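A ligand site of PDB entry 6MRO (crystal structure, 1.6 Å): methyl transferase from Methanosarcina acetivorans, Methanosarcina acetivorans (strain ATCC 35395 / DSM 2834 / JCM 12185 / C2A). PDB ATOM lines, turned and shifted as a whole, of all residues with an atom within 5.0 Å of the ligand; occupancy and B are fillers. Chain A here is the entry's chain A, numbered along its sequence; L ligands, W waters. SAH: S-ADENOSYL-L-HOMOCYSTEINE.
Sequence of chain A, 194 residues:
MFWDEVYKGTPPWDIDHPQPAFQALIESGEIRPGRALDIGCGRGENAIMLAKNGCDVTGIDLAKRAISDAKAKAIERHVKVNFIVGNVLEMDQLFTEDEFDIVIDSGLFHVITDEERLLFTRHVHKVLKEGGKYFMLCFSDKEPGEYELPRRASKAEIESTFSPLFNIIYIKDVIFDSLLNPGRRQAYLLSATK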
ATOM      1  N   TRP A   3      -0.965 -15.159 -18.429  1.00  0.00           N
ATOM      2  CA  TRP A   3      -1.458 -16.526 -18.331  1.00  0.00           C
ATOM      3  C   TRP A   3      -2.917 -16.662 -18.746  1.00  0.00           C
ATOM      4  O   TRP A   3      -3.307 -17.737 -19.207  1.00  0.00           O
ATOM      5  CB  TRP A   3      -1.208 -17.041 -16.921  1.00  0.00           C
ATOM      6  CG  TRP A   3       0.266 -17.206 -16.700  1.00  0.00           C
ATOM      7  CD1 TRP A   3       1.090 -16.402 -15.954  1.00  0.00           C
ATOM      8  CD2 TRP A   3       1.113 -18.211 -17.278  1.00  0.00           C
ATOM      9  NE1 TRP A   3       2.386 -16.863 -16.014  1.00  0.00           N
ATOM     10  CE2 TRP A   3       2.428 -17.977 -16.820  1.00  0.00           C
ATOM     11  CE3 TRP A   3       0.882 -19.295 -18.132  1.00  0.00           C
ATOM     12  CZ2 TRP A   3       3.507 -18.781 -17.195  1.00  0.00           C
ATOM     13  CZ3 TRP A   3       1.954 -20.099 -18.484  1.00  0.00           C
ATOM     14  CH2 TRP A   3       3.257 -19.831 -18.016  1.00  0.00           C
ATOM     15  N   TYR A   7      -4.397 -19.482 -22.103  1.00  0.00           N
ATOM     16  CA  TYR A   7      -5.521 -20.391 -21.967  1.00  0.00           C
ATOM     17  C   TYR A   7      -6.698 -20.011 -22.858  1.00  0.00           C
ATOM     18  O   TYR A   7      -7.770 -20.608 -22.744  1.00  0.00           O
ATOM     19  CB  TYR A   7      -5.944 -20.505 -20.505  1.00  0.00           C
ATOM     20  CG  TYR A   7      -4.999 -21.452 -19.765  1.00  0.00           C
ATOM     21  CD1 TYR A   7      -4.016 -20.960 -18.928  1.00  0.00           C
ATOM     22  CD2 TYR A   7      -5.059 -22.820 -19.968  1.00  0.00           C
ATOM     23  CE1 TYR A   7      -3.124 -21.808 -18.266  1.00  0.00           C
ATOM     24  CE2 TYR A   7      -4.162 -23.701 -19.322  1.00  0.00           C
ATOM     25  CZ  TYR A   7      -3.209 -23.175 -18.472  1.00  0.00           C
ATOM     26  OH  TYR A   7      -2.332 -24.046 -17.832  1.00  0.00           O
ATOM     27  N   TRP A  13       1.148 -27.909 -23.126  1.00  0.00           N
ATOM     28  CA  TRP A  13       1.151 -28.784 -21.954  1.00  0.00           C
ATOM     29  C   TRP A  13      -0.245 -29.264 -21.580  1.00  0.00           C
ATOM     30  O   TRP A  13      -0.387 -30.130 -20.691  1.00  0.00           O
ATOM     31  CB  TRP A  13       1.768 -28.063 -20.741  1.00  0.00           C
ATOM     32  CG  TRP A  13       1.004 -26.807 -20.413  1.00  0.00           C
ATOM     33  CD1 TRP A  13      -0.119 -26.705 -19.634  1.00  0.00           C
ATOM     34  CD2 TRP A  13       1.297 -25.485 -20.874  1.00  0.00           C
ATOM     35  NE1 TRP A  13      -0.540 -25.394 -19.594  1.00  0.00           N
ATOM     36  CE2 TRP A  13       0.318 -24.627 -20.346  1.00  0.00           C
ATOM     37  CE3 TRP A  13       2.310 -24.936 -21.689  1.00  0.00           C
ATOM     38  CZ2 TRP A  13       0.310 -23.254 -20.595  1.00  0.00           C
ATOM     39  CZ3 TRP A  13       2.289 -23.569 -21.942  1.00  0.00           C
ATOM     40  CH2 TRP A  13       1.301 -22.743 -21.383  1.00  0.00           C
ATOM     41  N   ASP A  14      -1.296 -28.727 -22.221  1.00  0.00           N
ATOM     42  CA  ASP A  14      -2.664 -28.922 -21.739  1.00  0.00           C
ATOM     43  C   ASP A  14      -3.232 -30.218 -22.300  1.00  0.00           C
ATOM     44  O   ASP A  14      -4.196 -30.241 -23.069  1.00  0.00           O
ATOM     45  CB  ASP A  14      -3.504 -27.702 -22.104  1.00  0.00           C
ATOM     46  CG  ASP A  14      -4.870 -27.742 -21.481  1.00  0.00           C
ATOM     47  OD1 ASP A  14      -4.976 -28.283 -20.355  1.00  0.00           O
ATOM     48  OD2 ASP A  14      -5.814 -27.246 -22.134  1.00  0.00           O
ATOM     49  N   GLN A  19      -0.265 -36.303 -16.293  1.00  0.00           N
ATOM     50  CA  GLN A  19       1.071 -36.619 -16.779  1.00  0.00           C
ATOM     51  C   GLN A  19       1.463 -38.022 -16.327  1.00  0.00           C
ATOM     52  O   GLN A  19       1.265 -38.376 -15.158  1.00  0.00           O
ATOM     53  CB  GLN A  19       2.091 -35.598 -16.268  1.00  0.00           C
ATOM     54  CG  GLN A  19       2.056 -34.293 -17.044  1.00  0.00           C
ATOM     55  CD  GLN A  19       2.627 -34.439 -18.418  1.00  0.00           C
ATOM     56  OE1 GLN A  19       3.256 -35.450 -18.745  1.00  0.00           O
ATOM     57  NE2 GLN A  19       2.378 -33.458 -19.269  1.00  0.00           N
ATOM     58  N   ASP A  38      -1.467 -28.870  -5.828  1.00  0.00           N
ATOM     59  CA  ASP A  38      -0.926 -28.846  -7.177  1.00  0.00           C
ATOM     60  C   ASP A  38      -0.687 -27.379  -7.511  1.00  0.00           C
ATOM     61  O   ASP A  38      -1.643 -26.623  -7.704  1.00  0.00           O
ATOM     62  CB  ASP A  38      -1.894 -29.505  -8.163  1.00  0.00           C
ATOM     63  CG  ASP A  38      -1.349 -29.549  -9.599  1.00  0.00           C
ATOM     64  OD1 ASP A  38      -0.406 -28.813  -9.911  1.00  0.00           O
ATOM     65  OD2 ASP A  38      -1.887 -30.332 -10.437  1.00  0.00           O
ATOM     66  N   ILE A  39       0.592 -26.956  -7.546  1.00  0.00           N
ATOM     67  CA  ILE A  39       0.923 -25.554  -7.774  1.00  0.00           C
ATOM     68  C   ILE A  39       1.019 -25.319  -9.287  1.00  0.00           C
ATOM     69  O   ILE A  39       1.678 -26.071 -10.003  1.00  0.00           O
ATOM     70  CB  ILE A  39       2.222 -25.157  -7.039  1.00  0.00           C
ATOM     71  CG1 ILE A  39       3.383 -26.093  -7.350  1.00  0.00           C
ATOM     72  CG2 ILE A  39       2.001 -25.129  -5.531  1.00  0.00           C
ATOM     73  CD1 ILE A  39       4.730 -25.616  -6.723  1.00  0.00           C
ATOM     74  N   GLY A  40       0.325 -24.284  -9.773  1.00  0.00           N
ATOM     75  CA  GLY A  40       0.221 -24.075 -11.203  1.00  0.00           C
ATOM     76  C   GLY A  40      -0.544 -25.206 -11.857  1.00  0.00           C
ATOM     77  O   GLY A  40      -0.076 -25.793 -12.831  1.00  0.00           O
ATOM     78  N   CYS A  41      -1.737 -25.498 -11.330  1.00  0.00           N
ATOM     79  CA  CYS A  41      -2.434 -26.730 -11.672  1.00  0.00           C
ATOM     80  C   CYS A  41      -3.072 -26.705 -13.057  1.00  0.00           C
ATOM     81  O   CYS A  41      -3.532 -27.761 -13.509  1.00  0.00           O
ATOM     82  CB  CYS A  41      -3.508 -27.020 -10.623  1.00  0.00           C
ATOM     83  SG  CYS A  41      -4.807 -25.732 -10.571  1.00  0.00           S
ATOM     84  N   GLY A  42      -3.154 -25.562 -13.719  1.00  0.00           N
ATOM     85  CA  GLY A  42      -3.755 -25.550 -15.042  1.00  0.00           C
ATOM     86  C   GLY A  42      -5.193 -26.048 -15.002  1.00  0.00           C
ATOM     87  O   GLY A  42      -5.949 -25.776 -14.062  1.00  0.00           O
ATOM     88  N   ASN A  46      -3.869 -33.456 -13.308  1.00  0.00           N
ATOM     89  CA  ASN A  46      -3.117 -34.113 -12.247  1.00  0.00           C
ATOM     90  C   ASN A  46      -3.825 -33.999 -10.912  1.00  0.00           C
ATOM     91  O   ASN A  46      -3.815 -34.933 -10.112  1.00  0.00           O
ATOM     92  CB  ASN A  46      -1.707 -33.526 -12.146  1.00  0.00           C
ATOM     93  CG  ASN A  46      -0.848 -33.872 -13.341  1.00  0.00           C
ATOM     94  OD1 ASN A  46      -0.906 -34.995 -13.844  1.00  0.00           O
ATOM     95  ND2 ASN A  46       0.010 -32.935 -13.770  1.00  0.00           N
ATOM     96  N   ILE A  60      -3.891 -24.568  -7.346  1.00  0.00           N
ATOM     97  CA  ILE A  60      -3.770 -23.120  -7.439  1.00  0.00           C
ATOM     98  C   ILE A  60      -3.169 -22.746  -8.789  1.00  0.00           C
ATOM     99  O   ILE A  60      -2.229 -23.398  -9.267  1.00  0.00           O
ATOM    100  CB  ILE A  60      -2.938 -22.558  -6.263  1.00  0.00           C
ATOM    101  CG1 ILE A  60      -2.782 -21.046  -6.392  1.00  0.00           C
ATOM    102  CG2 ILE A  60      -1.588 -23.296  -6.132  1.00  0.00           C
ATOM    103  CD1 ILE A  60      -2.254 -20.408  -5.150  1.00  0.00           C
ATOM    104  N   ASP A  61      -3.729 -21.716  -9.419  1.00  0.00           N
ATOM    105  CA  ASP A  61      -3.206 -21.261 -10.698  1.00  0.00           C
ATOM    106  C   ASP A  61      -3.573 -19.791 -10.875  1.00  0.00           C
ATOM    107  O   ASP A  61      -4.601 -19.346 -10.377  1.00  0.00           O
ATOM    108  CB  ASP A  61      -3.756 -22.098 -11.854  1.00  0.00           C
ATOM    109  CG  ASP A  61      -2.914 -21.979 -13.128  1.00  0.00           C
ATOM    110  OD1 ASP A  61      -2.951 -20.925 -13.795  1.00  0.00           O
ATOM    111  OD2 ASP A  61      -2.212 -22.964 -13.468  1.00  0.00           O
ATOM    112  N   LEU A  62      -2.716 -19.072 -11.594  1.00  0.00           N
ATOM    113  CA  LEU A  62      -2.951 -17.648 -11.860  1.00  0.00           C
ATOM    114  C   LEU A  62      -4.118 -17.426 -12.813  1.00  0.00           C
ATOM    115  O   LEU A  62      -4.793 -16.392 -12.741  1.00  0.00           O
ATOM    116  CB  LEU A  62      -1.685 -17.019 -12.441  1.00  0.00           C
ATOM    117  CG  LEU A  62      -0.608 -16.519 -11.493  1.00  0.00           C
ATOM    118  CD1 LEU A  62       0.584 -16.027 -12.317  1.00  0.00           C
ATOM    119  CD2 LEU A  62      -1.165 -15.407 -10.606  1.00  0.00           C
ATOM    120  N   ALA A  63      -4.380 -18.362 -13.709  1.00  0.00           N
ATOM    121  CA  ALA A  63      -5.309 -18.150 -14.819  1.00  0.00           C
ATOM    122  C   ALA A  63      -6.724 -18.528 -14.390  1.00  0.00           C
ATOM    123  O   ALA A  63      -7.000 -19.701 -14.136  1.00  0.00           O
ATOM    124  CB  ALA A  63      -4.879 -18.983 -16.017  1.00  0.00           C
ATOM    125  N   GLY A  86      -4.844 -17.993  -7.797  1.00  0.00           N
ATOM    126  CA  GLY A  86      -3.874 -17.450  -6.866  1.00  0.00           C
ATOM    127  C   GLY A  86      -2.464 -17.539  -7.410  1.00  0.00           C
ATOM    128  O   GLY A  86      -2.188 -18.196  -8.418  1.00  0.00           O
ATOM    129  N   ASN A  87      -1.567 -16.859  -6.695  1.00  0.00           N
ATOM    130  CA  ASN A  87      -0.166 -16.735  -7.049  1.00  0.00           C
ATOM    131  C   ASN A  87       0.667 -17.550  -6.072  1.00  0.00           C
ATOM    132  O   ASN A  87       0.621 -17.307  -4.870  1.00  0.00           O
ATOM    133  CB  ASN A  87       0.268 -15.273  -7.001  1.00  0.00           C
ATOM    134  CG  ASN A  87       1.586 -15.031  -7.676  1.00  0.00           C
ATOM    135  OD1 ASN A  87       2.467 -15.889  -7.696  1.00  0.00           O
ATOM    136  ND2 ASN A  87       1.734 -13.831  -8.242  1.00  0.00           N
ATOM    137  N   VAL A  88       1.435 -18.515  -6.593  1.00  0.00           N
ATOM    138  CA  VAL A  88       2.256 -19.365  -5.739  1.00  0.00           C
ATOM    139  C   VAL A  88       3.291 -18.538  -4.996  1.00  0.00           C
ATOM    140  O   VAL A  88       3.670 -18.874  -3.866  1.00  0.00           O
ATOM    141  CB  VAL A  88       2.886 -20.483  -6.588  1.00  0.00           C
ATOM    142  CG1 VAL A  88       4.056 -21.163  -5.850  1.00  0.00           C
ATOM    143  CG2 VAL A  88       1.817 -21.521  -6.951  1.00  0.00           C
ATOM    144  N   LEU A  89       3.742 -17.436  -5.586  1.00  0.00           N
ATOM    145  CA  LEU A  89       4.692 -16.533  -4.940  1.00  0.00           C
ATOM    146  C   LEU A  89       4.044 -15.694  -3.846  1.00  0.00           C
ATOM    147  O   LEU A  89       4.757 -14.929  -3.187  1.00  0.00           O
ATOM    148  CB  LEU A  89       5.337 -15.621  -5.977  1.00  0.00           C
ATOM    149  CG  LEU A  89       6.065 -16.303  -7.144  1.00  0.00           C
ATOM    150  CD1 LEU A  89       6.682 -15.268  -8.078  1.00  0.00           C
ATOM    151  CD2 LEU A  89       7.133 -17.266  -6.632  1.00  0.00           C
ATOM    152  N   SER A 106       3.839 -29.628 -11.992  1.00  0.00           N
ATOM    153  CA  SER A 106       3.871 -30.213 -13.336  1.00  0.00           C
ATOM    154  C   SER A 106       4.066 -29.042 -14.297  1.00  0.00           C
ATOM    155  O   SER A 106       3.101 -28.486 -14.812  1.00  0.00           O
ATOM    156  CB  SER A 106       2.558 -31.004 -13.632  1.00  0.00           C
ATOM    157  OG  SER A 106       2.510 -31.516 -14.969  1.00  0.00           O
ATOM    158  N   GLY A 107       5.326 -28.671 -14.516  1.00  0.00           N
ATOM    159  CA  GLY A 107       5.633 -27.566 -15.411  1.00  0.00           C
ATOM    160  C   GLY A 107       5.609 -26.159 -14.845  1.00  0.00           C
ATOM    161  O   GLY A 107       5.799 -25.197 -15.617  1.00  0.00           O
ATOM    162  N   LEU A 108       5.384 -25.979 -13.532  1.00  0.00           N
ATOM    163  CA  LEU A 108       5.422 -24.616 -12.991  1.00  0.00           C
ATOM    164  C   LEU A 108       6.867 -24.151 -12.766  1.00  0.00           C
ATOM    165  O   LEU A 108       7.253 -23.062 -13.222  1.00  0.00           O
ATOM    166  CB  LEU A 108       4.620 -24.520 -11.691  1.00  0.00           C
ATOM    167  CG  LEU A 108       4.706 -23.151 -10.984  1.00  0.00           C
ATOM    168  CD1 LEU A 108       4.255 -22.000 -11.921  1.00  0.00           C
ATOM    169  CD2 LEU A 108       3.901 -23.116  -9.655  1.00  0.00           C
ATOM    170  N   VAL A 111       8.543 -22.537 -15.580  1.00  0.00           N
ATOM    171  CA  VAL A 111       8.261 -21.172 -16.031  1.00  0.00           C
ATOM    172  C   VAL A 111       8.629 -20.112 -15.015  1.00  0.00           C
ATOM    173  O   VAL A 111       8.658 -18.928 -15.369  1.00  0.00           O
ATOM    174  CB  VAL A 111       6.781 -21.010 -16.449  1.00  0.00           C
ATOM    175  CG1 VAL A 111       6.427 -21.995 -17.537  1.00  0.00           C
ATOM    176  CG2 VAL A 111       5.852 -21.167 -15.260  1.00  0.00           C
ATOM    177  N   ILE A 112       8.919 -20.487 -13.762  1.00  0.00           N
ATOM    178  CA  ILE A 112       9.343 -19.525 -12.764  1.00  0.00           C
ATOM    179  C   ILE A 112      10.648 -18.873 -13.211  1.00  0.00           C
ATOM    180  O   ILE A 112      11.607 -19.559 -13.581  1.00  0.00           O
ATOM    181  CB  ILE A 112       9.488 -20.224 -11.402  1.00  0.00           C
ATOM    182  CG1 ILE A 112       8.131 -20.721 -10.906  1.00  0.00           C
ATOM    183  CG2 ILE A 112      10.120 -19.279 -10.354  1.00  0.00           C
ATOM    184  CD1 ILE A 112       7.109 -19.601 -10.636  1.00  0.00           C
HETATM  185  N   SAH L   1       0.274 -28.095 -14.243  1.00  0.00           N
HETATM  186  CA  SAH L   1      -0.550 -27.863 -15.437  1.00  0.00           C
HETATM  187  CB  SAH L   1      -0.194 -26.537 -16.096  1.00  0.00           C
HETATM  188  CG  SAH L   1       1.306 -26.368 -16.362  1.00  0.00           C
HETATM  189  SD  SAH L   1       1.713 -24.882 -17.312  1.00  0.00           S
HETATM  190  C   SAH L   1      -0.411 -28.985 -16.453  1.00  0.00           C
HETATM  191  O   SAH L   1       0.445 -29.877 -16.298  1.00  0.00           O
HETATM  192  OXT SAH L   1      -1.142 -29.006 -17.461  1.00  0.00           O
HETATM  193  C5' SAH L   1       2.209 -23.845 -15.902  1.00  0.00           C
HETATM  194  C4' SAH L   1       1.016 -23.263 -15.136  1.00  0.00           C
HETATM  195  O4' SAH L   1       1.503 -22.467 -14.062  1.00  0.00           O
HETATM  196  C3' SAH L   1       0.070 -22.391 -15.962  1.00  0.00           C
HETATM  197  O3' SAH L   1      -1.242 -22.911 -15.810  1.00  0.00           O
HETATM  198  C2' SAH L   1       0.250 -21.004 -15.359  1.00  0.00           C
HETATM  199  O2' SAH L   1      -0.920 -20.198 -15.379  1.00  0.00           O
HETATM  200  C1' SAH L   1       0.684 -21.321 -13.941  1.00  0.00           C
HETATM  201  N9  SAH L   1       1.467 -20.288 -13.261  1.00  0.00           N
HETATM  202  C8  SAH L   1       2.552 -19.585 -13.749  1.00  0.00           C
HETATM  203  N7  SAH L   1       2.994 -18.772 -12.773  1.00  0.00           N
HETATM  204  C5  SAH L   1       2.231 -18.959 -11.676  1.00  0.00           C
HETATM  205  C6  SAH L   1       2.238 -18.397 -10.401  1.00  0.00           C
HETATM  206  N6  SAH L   1       3.127 -17.463 -10.081  1.00  0.00           N
HETATM  207  N1  SAH L   1       1.310 -18.802  -9.480  1.00  0.00           N
HETATM  208  C2  SAH L   1       0.375 -19.771  -9.804  1.00  0.00           C
HETATM  209  N3  SAH L   1       0.350 -20.321 -11.071  1.00  0.00           N
HETATM  210  C4  SAH L   1       1.284 -19.923 -11.969  1.00  0.00           C
HETATM  211  O   HOH W   1      -2.752 -31.290 -18.542  1.00  0.00           O
HETATM  212  O   HOH W   2      -3.585 -27.722 -17.961  1.00  0.00           O
HETATM  213  O   HOH W   3       1.540 -28.255 -11.640  1.00  0.00           O
HETATM  214  O   HOH W   4       0.760 -31.266 -18.471  1.00  0.00           O
HETATM  215  O   HOH W   5      -0.815 -30.357 -12.908  1.00  0.00           O
HETATM  216  O   HOH W   6       4.762 -25.194 -18.334  1.00  0.00           O
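O of Gly 40 lies within hydrogen-bond range of N of the ligand, 2.7 Å away. The indole nitrogen (NE1) of Trp 13 sits close to a sulfur (SD) of the ligand, 3.2 Å away. OD2 of Asp 61 sits at hydrogen-bond distance from O3' of the ligand. N1 of the ligand sits at hydrogen-bond distance from N of Val 88, 2.9 Å away. O of the ligand lies within hydrogen-bond range of OG of Ser 106, at 3.0 Å. The side-chain amide oxygen of Asn 87 sits at hydrogen-bond distance from a nitrogen (N6) of the ligand. O3' of the ligand is in hydrogen-bond range of OH of Tyr 7, 2.6 Å away. The backbone carbonyl oxygen (O) of Ser 106 lies within hydrogen-bond range of a nitrogen (N) of the ligand (2.9 Å). A nitrogen (N3) of the ligand sits at hydrogen-bond distance from the backbone NH (N) of Leu 62 (3.4 Å).
O of Ile 60 lies within hydrogen-bond range of N of Gly 40. N of Ala 63 sits at hydrogen-bond distance from OD1 of Asp 61, at 2.9 Å. The backbone carbonyl oxygen (O) of Gly 86 lies within hydrogen-bond range of the backbone NH (N) of Leu 62, at 3.3 Å. The side-chain hydroxyl of Tyr 7 sits at hydrogen-bond distance from the indole nitrogen of Trp 13 (2.9 Å). The backbone NH of Cys 41 is in hydrogen-bond range of the backbone carbonyl oxygen of Ile 60. N of Gly 86 sits at hydrogen-bond distance from O of Asp 61. The side-chain amide oxygen (OD1) of Asn 87 sits at hydrogen-bond distance from the backbone NH (N) of Leu 89, 2.9 Å away. OG of Ser 106 sits at hydrogen-bond distance from ND2 of Asn 46, 3.1 Å away.
Trp 3 touches the ligand (CE3 to C2', 3.3 Å). Cys 41 touches the ligand. CA of Gly 42 touches O3' of the ligand, 3.7 Å away. ND2 of Asn 46 touches O of the ligand (3.99 Å). Gly 86 touches the ligand. Gly 107 touches the ligand (O to C5', 3.8 Å). Leu 108 touches the ligand. Val 111 touches the ligand. Within 4 Å of the ligand: Trp 3, Tyr 7, Trp 13, Gly 40, Cys 41, Gly 42, Asn 46, Asp 61, Leu 62, Gly 86, Asn 87, Val 88, Ser 106, Gly 107, Leu 108 and Val 111. The nearest printed residue that does not touch the ligand is Ala 63 (4.2 Å).
Water W4 lies within hydrogen-bond range of an oxygen (O) of the ligand, the backbone carbonyl oxygen of Trp 13 and the side-chain amide nitrogen of Gln 19. Water W2 lies within hydrogen-bond range of OXT of the ligand (2.8 Å) and OD1 of Asp 14 (2.8 Å). Water W5 lies within hydrogen-bond range of OD2 of Asp 38 (2.7 Å), ND2 of Asn 46 (2.8 Å) and N of the ligand (2.8 Å). Water W1 lies within hydrogen-bond range of an oxygen (OXT) of the ligand and the backbone carbonyl oxygen of Trp 13. Water W6 lies within hydrogen-bond range of O of Gly 107 (2.9 Å) and SD of the ligand (3.2 Å).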
